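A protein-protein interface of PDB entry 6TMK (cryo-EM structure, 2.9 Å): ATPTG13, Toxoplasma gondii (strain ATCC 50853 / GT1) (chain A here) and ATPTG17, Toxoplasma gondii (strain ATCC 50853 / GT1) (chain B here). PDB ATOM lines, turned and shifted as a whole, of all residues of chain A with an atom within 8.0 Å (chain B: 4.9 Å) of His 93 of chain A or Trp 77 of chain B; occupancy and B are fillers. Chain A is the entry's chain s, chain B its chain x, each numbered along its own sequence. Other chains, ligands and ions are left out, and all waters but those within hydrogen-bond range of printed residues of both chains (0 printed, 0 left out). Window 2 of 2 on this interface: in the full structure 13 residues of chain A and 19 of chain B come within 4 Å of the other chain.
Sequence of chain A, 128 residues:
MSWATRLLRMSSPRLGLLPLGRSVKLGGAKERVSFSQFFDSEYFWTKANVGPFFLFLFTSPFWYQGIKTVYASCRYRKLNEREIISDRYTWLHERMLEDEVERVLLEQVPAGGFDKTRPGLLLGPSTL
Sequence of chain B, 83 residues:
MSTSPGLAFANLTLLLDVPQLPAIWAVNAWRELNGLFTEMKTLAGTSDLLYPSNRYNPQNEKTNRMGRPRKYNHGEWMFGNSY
Of the 15 printed residues of chain A, 5 touch a printed residue of chain B.
Of the 9 printed residues of chain B, 5 touch a printed residue of chain A.
Among the printed residues, no Asp or Glu carboxylate lies within 4 Å of a Lys or Arg side-chain nitrogen of the other chain.
NE1 of Trp 77 of chain B sits close to SD of Met 96 of chain A (3.4 Å).
The side-chain hydroxyl (OG1) of Thr 90 of chain A sits at hydrogen-bond distance from the backbone carbonyl oxygen (O) of Ser 82 of chain B (2.8 Å).
O of Ser 86 of chain A is in hydrogen-bond range of OG1 of Thr 90 of chain A.
Among the printed residues, merely in contact across the chains: His 93 of chain A with Tyr 72 of chain B, Tyr 89 of chain A with Trp 77 of chain B, His 93 of chain A with Ser 82 of chain B, His 93 of chain A with Trp 77 of chain B, Met 96 of chain A with Phe 79 of chain B, Met 96 of chain A with Met 78 of chain B and Leu 97 of chain A with Tyr 72 of chain B.
Ser 86 of chain A touches none of the printed residues of chain B.
Of the printed residues of chain B, Tyr 89 of chain A touches Trp 77 (3.5 Å).
Printed residues of chain B within 4 Å of Thr 90 of chain A: Ser 82.
His 93 of chain A touches three residues of chain B.
Of the printed residues of chain B, Met 96 of chain A touches Trp 77 (3.4 Å), Met 78 (3.8 Å) and Phe 79 (3.7 Å).
Of the printed residues of chain A, Tyr 72 of chain B touches His 93 (3.2 Å) and Leu 97 (3.9 Å).
Of the printed residues of chain A, Trp 77 of chain B touches Tyr 89 (3.5 Å), His 93 (3.7 Å) and Met 96 (3.4 Å).
Asn 81 of chain B touches none of the printed residues of chain A.
The nearest printed residue of chain B that does not touch His 93 of chain A is Glu 76 of chain B (6.2 Å).
The nearest residue of chain A that does not touch Trp 77 of chain B is Leu 92 of chain A (4.3 Å).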
ATOM      1  N   SER A  86     -27.366 -23.867 -23.190  1.00  0.00           N
ATOM      2  CA  SER A  86     -26.577 -24.596 -22.208  1.00  0.00           C
ATOM      3  C   SER A  86     -26.373 -23.767 -20.949  1.00  0.00           C
ATOM      4  O   SER A  86     -26.517 -24.270 -19.826  1.00  0.00           O
ATOM      5  CB  SER A  86     -25.243 -24.993 -22.829  1.00  0.00           C
ATOM      6  OG  SER A  86     -24.382 -25.594 -21.884  1.00  0.00           O
ATOM      7  N   ASP A  87     -26.025 -22.494 -21.118  1.00  0.00           N
ATOM      8  CA  ASP A  87     -25.827 -21.637 -19.959  1.00  0.00           C
ATOM      9  C   ASP A  87     -27.117 -21.490 -19.167  1.00  0.00           C
ATOM     10  O   ASP A  87     -27.104 -21.502 -17.927  1.00  0.00           O
ATOM     11  CB  ASP A  87     -25.307 -20.277 -20.406  1.00  0.00           C
ATOM     12  CG  ASP A  87     -23.896 -20.344 -20.948  1.00  0.00           C
ATOM     13  OD1 ASP A  87     -23.580 -19.571 -21.877  1.00  0.00           O
ATOM     14  OD2 ASP A  87     -23.103 -21.174 -20.456  1.00  0.00           O
ATOM     15  N   ARG A  88     -28.249 -21.376 -19.861  1.00  0.00           N
ATOM     16  CA  ARG A  88     -29.516 -21.251 -19.152  1.00  0.00           C
ATOM     17  C   ARG A  88     -29.892 -22.541 -18.433  1.00  0.00           C
ATOM     18  O   ARG A  88     -30.477 -22.493 -17.345  1.00  0.00           O
ATOM     19  CB  ARG A  88     -30.602 -20.822 -20.121  1.00  0.00           C
ATOM     20  CG  ARG A  88     -30.445 -19.405 -20.546  1.00  0.00           C
ATOM     21  CD  ARG A  88     -31.505 -18.965 -21.494  1.00  0.00           C
ATOM     22  NE  ARG A  88     -31.301 -17.589 -21.915  1.00  0.00           N
ATOM     23  CZ  ARG A  88     -32.077 -16.956 -22.780  1.00  0.00           C
ATOM     24  NH1 ARG A  88     -33.112 -17.576 -23.309  1.00  0.00           N
ATOM     25  NH2 ARG A  88     -31.820 -15.704 -23.109  1.00  0.00           N
ATOM     26  N   TYR A  89     -29.552 -23.697 -19.002  1.00  0.00           N
ATOM     27  CA  TYR A  89     -29.807 -24.956 -18.310  1.00  0.00           C
ATOM     28  C   TYR A  89     -28.951 -25.081 -17.058  1.00  0.00           C
ATOM     29  O   TYR A  89     -29.411 -25.594 -16.034  1.00  0.00           O
ATOM     30  CB  TYR A  89     -29.563 -26.135 -19.244  1.00  0.00           C
ATOM     31  CG  TYR A  89     -30.790 -26.580 -19.996  1.00  0.00           C
ATOM     32  CD1 TYR A  89     -31.881 -27.100 -19.328  1.00  0.00           C
ATOM     33  CD2 TYR A  89     -30.857 -26.485 -21.370  1.00  0.00           C
ATOM     34  CE1 TYR A  89     -32.997 -27.507 -20.004  1.00  0.00           C
ATOM     35  CE2 TYR A  89     -31.971 -26.890 -22.052  1.00  0.00           C
ATOM     36  CZ  TYR A  89     -33.040 -27.400 -21.365  1.00  0.00           C
ATOM     37  OH  TYR A  89     -34.159 -27.811 -22.042  1.00  0.00           O
ATOM     38  N   THR A  90     -27.704 -24.621 -17.122  1.00  0.00           N
ATOM     39  CA  THR A  90     -26.851 -24.636 -15.936  1.00  0.00           C
ATOM     40  C   THR A  90     -27.433 -23.746 -14.844  1.00  0.00           C
ATOM     41  O   THR A  90     -27.492 -24.125 -13.662  1.00  0.00           O
ATOM     42  CB  THR A  90     -25.444 -24.180 -16.313  1.00  0.00           C
ATOM     43  OG1 THR A  90     -24.941 -24.990 -17.377  1.00  0.00           O
ATOM     44  CG2 THR A  90     -24.524 -24.303 -15.141  1.00  0.00           C
ATOM     45  N   TRP A  91     -27.854 -22.542 -15.228  1.00  0.00           N
ATOM     46  CA  TRP A  91     -28.551 -21.649 -14.313  1.00  0.00           C
ATOM     47  C   TRP A  91     -29.733 -22.348 -13.647  1.00  0.00           C
ATOM     48  O   TRP A  91     -29.881 -22.320 -12.416  1.00  0.00           O
ATOM     49  CB  TRP A  91     -28.993 -20.418 -15.104  1.00  0.00           C
ATOM     50  CG  TRP A  91     -29.825 -19.438 -14.373  1.00  0.00           C
ATOM     51  CD1 TRP A  91     -29.391 -18.435 -13.574  1.00  0.00           C
ATOM     52  CD2 TRP A  91     -31.249 -19.342 -14.402  1.00  0.00           C
ATOM     53  NE1 TRP A  91     -30.453 -17.726 -13.086  1.00  0.00           N
ATOM     54  CE2 TRP A  91     -31.609 -18.265 -13.582  1.00  0.00           C
ATOM     55  CE3 TRP A  91     -32.255 -20.068 -15.037  1.00  0.00           C
ATOM     56  CZ2 TRP A  91     -32.928 -17.898 -13.378  1.00  0.00           C
ATOM     57  CZ3 TRP A  91     -33.556 -19.704 -14.833  1.00  0.00           C
ATOM     58  CH2 TRP A  91     -33.885 -18.629 -14.012  1.00  0.00           C
ATOM     59  N   LEU A  92     -30.590 -22.975 -14.451  1.00  0.00           N
ATOM     60  CA  LEU A  92     -31.765 -23.649 -13.913  1.00  0.00           C
ATOM     61  C   LEU A  92     -31.385 -24.773 -12.959  1.00  0.00           C
ATOM     62  O   LEU A  92     -32.052 -24.986 -11.941  1.00  0.00           O
ATOM     63  CB  LEU A  92     -32.603 -24.190 -15.060  1.00  0.00           C
ATOM     64  CG  LEU A  92     -33.899 -24.890 -14.688  1.00  0.00           C
ATOM     65  CD1 LEU A  92     -34.841 -23.928 -14.030  1.00  0.00           C
ATOM     66  CD2 LEU A  92     -34.505 -25.470 -15.921  1.00  0.00           C
ATOM     67  N   HIS A  93     -30.334 -25.519 -13.287  1.00  0.00           N
ATOM     68  CA  HIS A  93     -29.859 -26.585 -12.415  1.00  0.00           C
ATOM     69  C   HIS A  93     -29.511 -26.044 -11.037  1.00  0.00           C
ATOM     70  O   HIS A  93     -29.947 -26.578 -10.005  1.00  0.00           O
ATOM     71  CB  HIS A  93     -28.653 -27.249 -13.071  1.00  0.00           C
ATOM     72  CG  HIS A  93     -28.094 -28.409 -12.313  1.00  0.00           C
ATOM     73  ND1 HIS A  93     -26.748 -28.552 -12.068  1.00  0.00           N
ATOM     74  CD2 HIS A  93     -28.692 -29.492 -11.768  1.00  0.00           C
ATOM     75  CE1 HIS A  93     -26.542 -29.667 -11.393  1.00  0.00           C
ATOM     76  NE2 HIS A  93     -27.707 -30.257 -11.198  1.00  0.00           N
ATOM     77  N   GLU A  94     -28.728 -24.968 -11.006  1.00  0.00           N
ATOM     78  CA  GLU A  94     -28.329 -24.391  -9.727  1.00  0.00           C
ATOM     79  C   GLU A  94     -29.539 -23.894  -8.946  1.00  0.00           C
ATOM     80  O   GLU A  94     -29.627 -24.084  -7.723  1.00  0.00           O
ATOM     81  CB  GLU A  94     -27.340 -23.264  -9.969  1.00  0.00           C
ATOM     82  CG  GLU A  94     -25.964 -23.752 -10.303  1.00  0.00           C
ATOM     83  CD  GLU A  94     -25.204 -22.799 -11.198  1.00  0.00           C
ATOM     84  OE1 GLU A  94     -25.577 -21.609 -11.259  1.00  0.00           O
ATOM     85  OE2 GLU A  94     -24.235 -23.242 -11.847  1.00  0.00           O
ATOM     86  N   ARG A  95     -30.489 -23.266  -9.636  1.00  0.00           N
ATOM     87  CA  ARG A  95     -31.659 -22.743  -8.943  1.00  0.00           C
ATOM     88  C   ARG A  95     -32.524 -23.867  -8.386  1.00  0.00           C
ATOM     89  O   ARG A  95     -33.097 -23.739  -7.298  1.00  0.00           O
ATOM     90  CB  ARG A  95     -32.464 -21.864  -9.892  1.00  0.00           C
ATOM     91  CG  ARG A  95     -31.693 -20.694 -10.445  1.00  0.00           C
ATOM     92  CD  ARG A  95     -31.395 -19.635  -9.409  1.00  0.00           C
ATOM     93  NE  ARG A  95     -30.225 -19.929  -8.592  1.00  0.00           N
ATOM     94  CZ  ARG A  95     -28.977 -19.947  -9.046  1.00  0.00           C
ATOM     95  NH1 ARG A  95     -27.978 -20.217  -8.224  1.00  0.00           N
ATOM     96  NH2 ARG A  95     -28.728 -19.699 -10.316  1.00  0.00           N
ATOM     97  N   MET A  96     -32.616 -24.984  -9.106  1.00  0.00           N
ATOM     98  CA  MET A  96     -33.387 -26.117  -8.611  1.00  0.00           C
ATOM     99  C   MET A  96     -32.733 -26.730  -7.380  1.00  0.00           C
ATOM    100  O   MET A  96     -33.423 -27.148  -6.439  1.00  0.00           O
ATOM    101  CB  MET A  96     -33.544 -27.153  -9.718  1.00  0.00           C
ATOM    102  CG  MET A  96     -34.486 -26.719 -10.819  1.00  0.00           C
ATOM    103  SD  MET A  96     -34.419 -27.759 -12.278  1.00  0.00           S
ATOM    104  CE  MET A  96     -35.528 -29.062 -11.781  1.00  0.00           C
ATOM    105  N   LEU A  97     -31.402 -26.782  -7.360  1.00  0.00           N
ATOM    106  CA  LEU A  97     -30.716 -27.246  -6.157  1.00  0.00           C
ATOM    107  C   LEU A  97     -30.999 -26.328  -4.974  1.00  0.00           C
ATOM    108  O   LEU A  97     -31.246 -26.794  -3.851  1.00  0.00           O
ATOM    109  CB  LEU A  97     -29.217 -27.338  -6.409  1.00  0.00           C
ATOM    110  CG  LEU A  97     -28.762 -28.362  -7.440  1.00  0.00           C
ATOM    111  CD1 LEU A  97     -27.275 -28.280  -7.630  1.00  0.00           C
ATOM    112  CD2 LEU A  97     -29.161 -29.750  -7.041  1.00  0.00           C
ATOM    113  N   GLU A  98     -30.962 -25.016  -5.205  1.00  0.00           N
ATOM    114  CA  GLU A  98     -31.313 -24.072  -4.151  1.00  0.00           C
ATOM    115  C   GLU A  98     -32.733 -24.305  -3.647  1.00  0.00           C
ATOM    116  O   GLU A  98     -32.998 -24.222  -2.442  1.00  0.00           O
ATOM    117  CB  GLU A  98     -31.174 -22.646  -4.668  1.00  0.00           C
ATOM    118  CG  GLU A  98     -29.760 -22.152  -4.783  1.00  0.00           C
ATOM    119  CD  GLU A  98     -29.686 -20.785  -5.427  1.00  0.00           C
ATOM    120  OE1 GLU A  98     -30.753 -20.189  -5.677  1.00  0.00           O
ATOM    121  OE2 GLU A  98     -28.563 -20.311  -5.695  1.00  0.00           O
ATOM    122  N   ASP A  99     -33.660 -24.590  -4.559  1.00  0.00           N
ATOM    123  CA  ASP A  99     -35.041 -24.831  -4.157  1.00  0.00           C
ATOM    124  C   ASP A  99     -35.155 -26.085  -3.303  1.00  0.00           C
ATOM    125  O   ASP A  99     -35.920 -26.117  -2.333  1.00  0.00           O
ATOM    126  CB  ASP A  99     -35.934 -24.936  -5.387  1.00  0.00           C
ATOM    127  CG  ASP A  99     -36.020 -23.634  -6.158  1.00  0.00           C
ATOM    128  OD1 ASP A  99     -35.706 -22.576  -5.575  1.00  0.00           O
ATOM    129  OD2 ASP A  99     -36.403 -23.667  -7.347  1.00  0.00           O
ATOM    130  N   GLU A 100     -34.406 -27.130  -3.648  1.00  0.00           N
ATOM    131  CA  GLU A 100     -34.399 -28.336  -2.826  1.00  0.00           C
ATOM    132  C   GLU A 100     -33.886 -28.034  -1.424  1.00  0.00           C
ATOM    133  O   GLU A 100     -34.457 -28.485  -0.419  1.00  0.00           O
ATOM    134  CB  GLU A 100     -33.544 -29.411  -3.486  1.00  0.00           C
ATOM    135  CG  GLU A 100     -33.545 -30.730  -2.749  1.00  0.00           C
ATOM    136  CD  GLU A 100     -32.778 -31.807  -3.489  1.00  0.00           C
ATOM    137  OE1 GLU A 100     -32.493 -32.863  -2.882  1.00  0.00           O
ATOM    138  OE2 GLU A 100     -32.458 -31.598  -4.678  1.00  0.00           O
ATOM    139  N   TYR B  72     -21.322 -29.936  -8.858  1.00  0.00           N
ATOM    140  CA  TYR B  72     -22.681 -30.465  -8.776  1.00  0.00           C
ATOM    141  C   TYR B  72     -22.952 -31.480  -9.880  1.00  0.00           C
ATOM    142  O   TYR B  72     -24.011 -31.475 -10.508  1.00  0.00           O
ATOM    143  CB  TYR B  72     -23.700 -29.328  -8.827  1.00  0.00           C
ATOM    144  CG  TYR B  72     -23.330 -28.152  -7.965  1.00  0.00           C
ATOM    145  CD1 TYR B  72     -22.936 -28.328  -6.654  1.00  0.00           C
ATOM    146  CD2 TYR B  72     -23.370 -26.865  -8.466  1.00  0.00           C
ATOM    147  CE1 TYR B  72     -22.592 -27.256  -5.867  1.00  0.00           C
ATOM    148  CE2 TYR B  72     -23.030 -25.790  -7.688  1.00  0.00           C
ATOM    149  CZ  TYR B  72     -22.643 -25.990  -6.387  1.00  0.00           C
ATOM    150  OH  TYR B  72     -22.297 -24.924  -5.595  1.00  0.00           O
ATOM    151  N   GLY B  75     -24.666 -36.381  -8.967  1.00  0.00           N
ATOM    152  CA  GLY B  75     -25.959 -36.997  -9.156  1.00  0.00           C
ATOM    153  C   GLY B  75     -26.462 -36.855 -10.581  1.00  0.00           C
ATOM    154  O   GLY B  75     -25.767 -36.381 -11.481  1.00  0.00           O
ATOM    155  N   GLU B  76     -27.704 -37.284 -10.778  1.00  0.00           N
ATOM    156  CA  GLU B  76     -28.371 -37.197 -12.066  1.00  0.00           C
ATOM    157  C   GLU B  76     -29.540 -36.226 -11.990  1.00  0.00           C
ATOM    158  O   GLU B  76     -30.118 -36.005 -10.922  1.00  0.00           O
ATOM    159  CB  GLU B  76     -28.866 -38.568 -12.515  1.00  0.00           C
ATOM    160  CG  GLU B  76     -28.994 -38.705 -14.011  1.00  0.00           C
ATOM    161  CD  GLU B  76     -27.649 -38.741 -14.706  1.00  0.00           C
ATOM    162  OE1 GLU B  76     -27.617 -38.680 -15.953  1.00  0.00           O
ATOM    163  OE2 GLU B  76     -26.621 -38.827 -14.003  1.00  0.00           O
ATOM    164  N   TRP B  77     -29.882 -35.647 -13.137  1.00  0.00           N
ATOM    165  CA  TRP B  77     -30.830 -34.547 -13.205  1.00  0.00           C
ATOM    166  C   TRP B  77     -31.934 -34.871 -14.199  1.00  0.00           C
ATOM    167  O   TRP B  77     -31.686 -35.484 -15.241  1.00  0.00           O
ATOM    168  CB  TRP B  77     -30.115 -33.259 -13.599  1.00  0.00           C
ATOM    169  CG  TRP B  77     -30.941 -32.036 -13.485  1.00  0.00           C
ATOM    170  CD1 TRP B  77     -31.869 -31.759 -12.536  1.00  0.00           C
ATOM    171  CD2 TRP B  77     -30.901 -30.903 -14.349  1.00  0.00           C
ATOM    172  NE1 TRP B  77     -32.419 -30.524 -12.757  1.00  0.00           N
ATOM    173  CE2 TRP B  77     -31.838 -29.979 -13.869  1.00  0.00           C
ATOM    174  CE3 TRP B  77     -30.164 -30.581 -15.486  1.00  0.00           C
ATOM    175  CZ2 TRP B  77     -32.057 -28.759 -14.484  1.00  0.00           C
ATOM    176  CZ3 TRP B  77     -30.385 -29.376 -16.093  1.00  0.00           C
ATOM    177  CH2 TRP B  77     -31.320 -28.477 -15.594  1.00  0.00           C
ATOM    178  N   MET B  78     -33.153 -34.443 -13.869  1.00  0.00           N
ATOM    179  CA  MET B  78     -34.316 -34.813 -14.667  1.00  0.00           C
ATOM    180  C   MET B  78     -34.233 -34.249 -16.079  1.00  0.00           C
ATOM    181  O   MET B  78     -34.635 -34.910 -17.043  1.00  0.00           O
ATOM    182  CB  MET B  78     -35.592 -34.343 -13.973  1.00  0.00           C
ATOM    183  CG  MET B  78     -35.639 -32.869 -13.665  1.00  0.00           C
ATOM    184  SD  MET B  78     -37.111 -32.407 -12.738  1.00  0.00           S
ATOM    185  CE  MET B  78     -38.347 -32.505 -14.024  1.00  0.00           C
ATOM    186  N   PHE B  79     -33.721 -33.033 -16.226  1.00  0.00           N
ATOM    187  CA  PHE B  79     -33.569 -32.417 -17.537  1.00  0.00           C
ATOM    188  C   PHE B  79     -32.314 -32.872 -18.263  1.00  0.00           C
ATOM    189  O   PHE B  79     -31.988 -32.318 -19.315  1.00  0.00           O
ATOM    190  CB  PHE B  79     -33.557 -30.895 -17.403  1.00  0.00           C
ATOM    191  CG  PHE B  79     -34.884 -30.312 -17.034  1.00  0.00           C
ATOM    192  CD1 PHE B  79     -35.893 -30.214 -17.967  1.00  0.00           C
ATOM    193  CD2 PHE B  79     -35.122 -29.867 -15.752  1.00  0.00           C
ATOM    194  CE1 PHE B  79     -37.111 -29.681 -17.626  1.00  0.00           C
ATOM    195  CE2 PHE B  79     -36.336 -29.334 -15.409  1.00  0.00           C
ATOM    196  CZ  PHE B  79     -37.334 -29.242 -16.345  1.00  0.00           C
ATOM    197  N   GLY B  80     -31.602 -33.848 -17.723  1.00  0.00           N
ATOM    198  CA  GLY B  80     -30.491 -34.466 -18.426  1.00  0.00           C
ATOM    199  C   GLY B  80     -29.160 -33.853 -18.023  1.00  0.00           C
ATOM    200  O   GLY B  80     -28.880 -33.680 -16.839  1.00  0.00           O
ATOM    201  N   ASN B  81     -28.338 -33.533 -19.017  1.00  0.00           N
ATOM    202  CA  ASN B  81     -27.061 -32.896 -18.744  1.00  0.00           C
ATOM    203  C   ASN B  81     -27.273 -31.532 -18.106  1.00  0.00           C
ATOM    204  O   ASN B  81     -28.261 -30.843 -18.366  1.00  0.00           O
ATOM    205  CB  ASN B  81     -26.251 -32.753 -20.025  1.00  0.00           C
ATOM    206  CG  ASN B  81     -25.655 -34.060 -20.483  1.00  0.00           C
ATOM    207  OD1 ASN B  81     -25.313 -34.917 -19.668  1.00  0.00           O
ATOM    208  ND2 ASN B  81     -25.519 -34.222 -21.792  1.00  0.00           N
ATOM    209  N   SER B  82     -26.319 -31.139 -17.273  1.00  0.00           N
ATOM    210  CA  SER B  82     -26.372 -29.866 -16.579  1.00  0.00           C
ATOM    211  C   SER B  82     -25.838 -28.722 -17.418  1.00  0.00           C
ATOM    212  O   SER B  82     -25.451 -27.687 -16.867  1.00  0.00           O
ATOM    213  CB  SER B  82     -25.582 -29.971 -15.280  1.00  0.00           C
ATOM    214  OG  SER B  82     -25.947 -31.135 -14.567  1.00  0.00           O
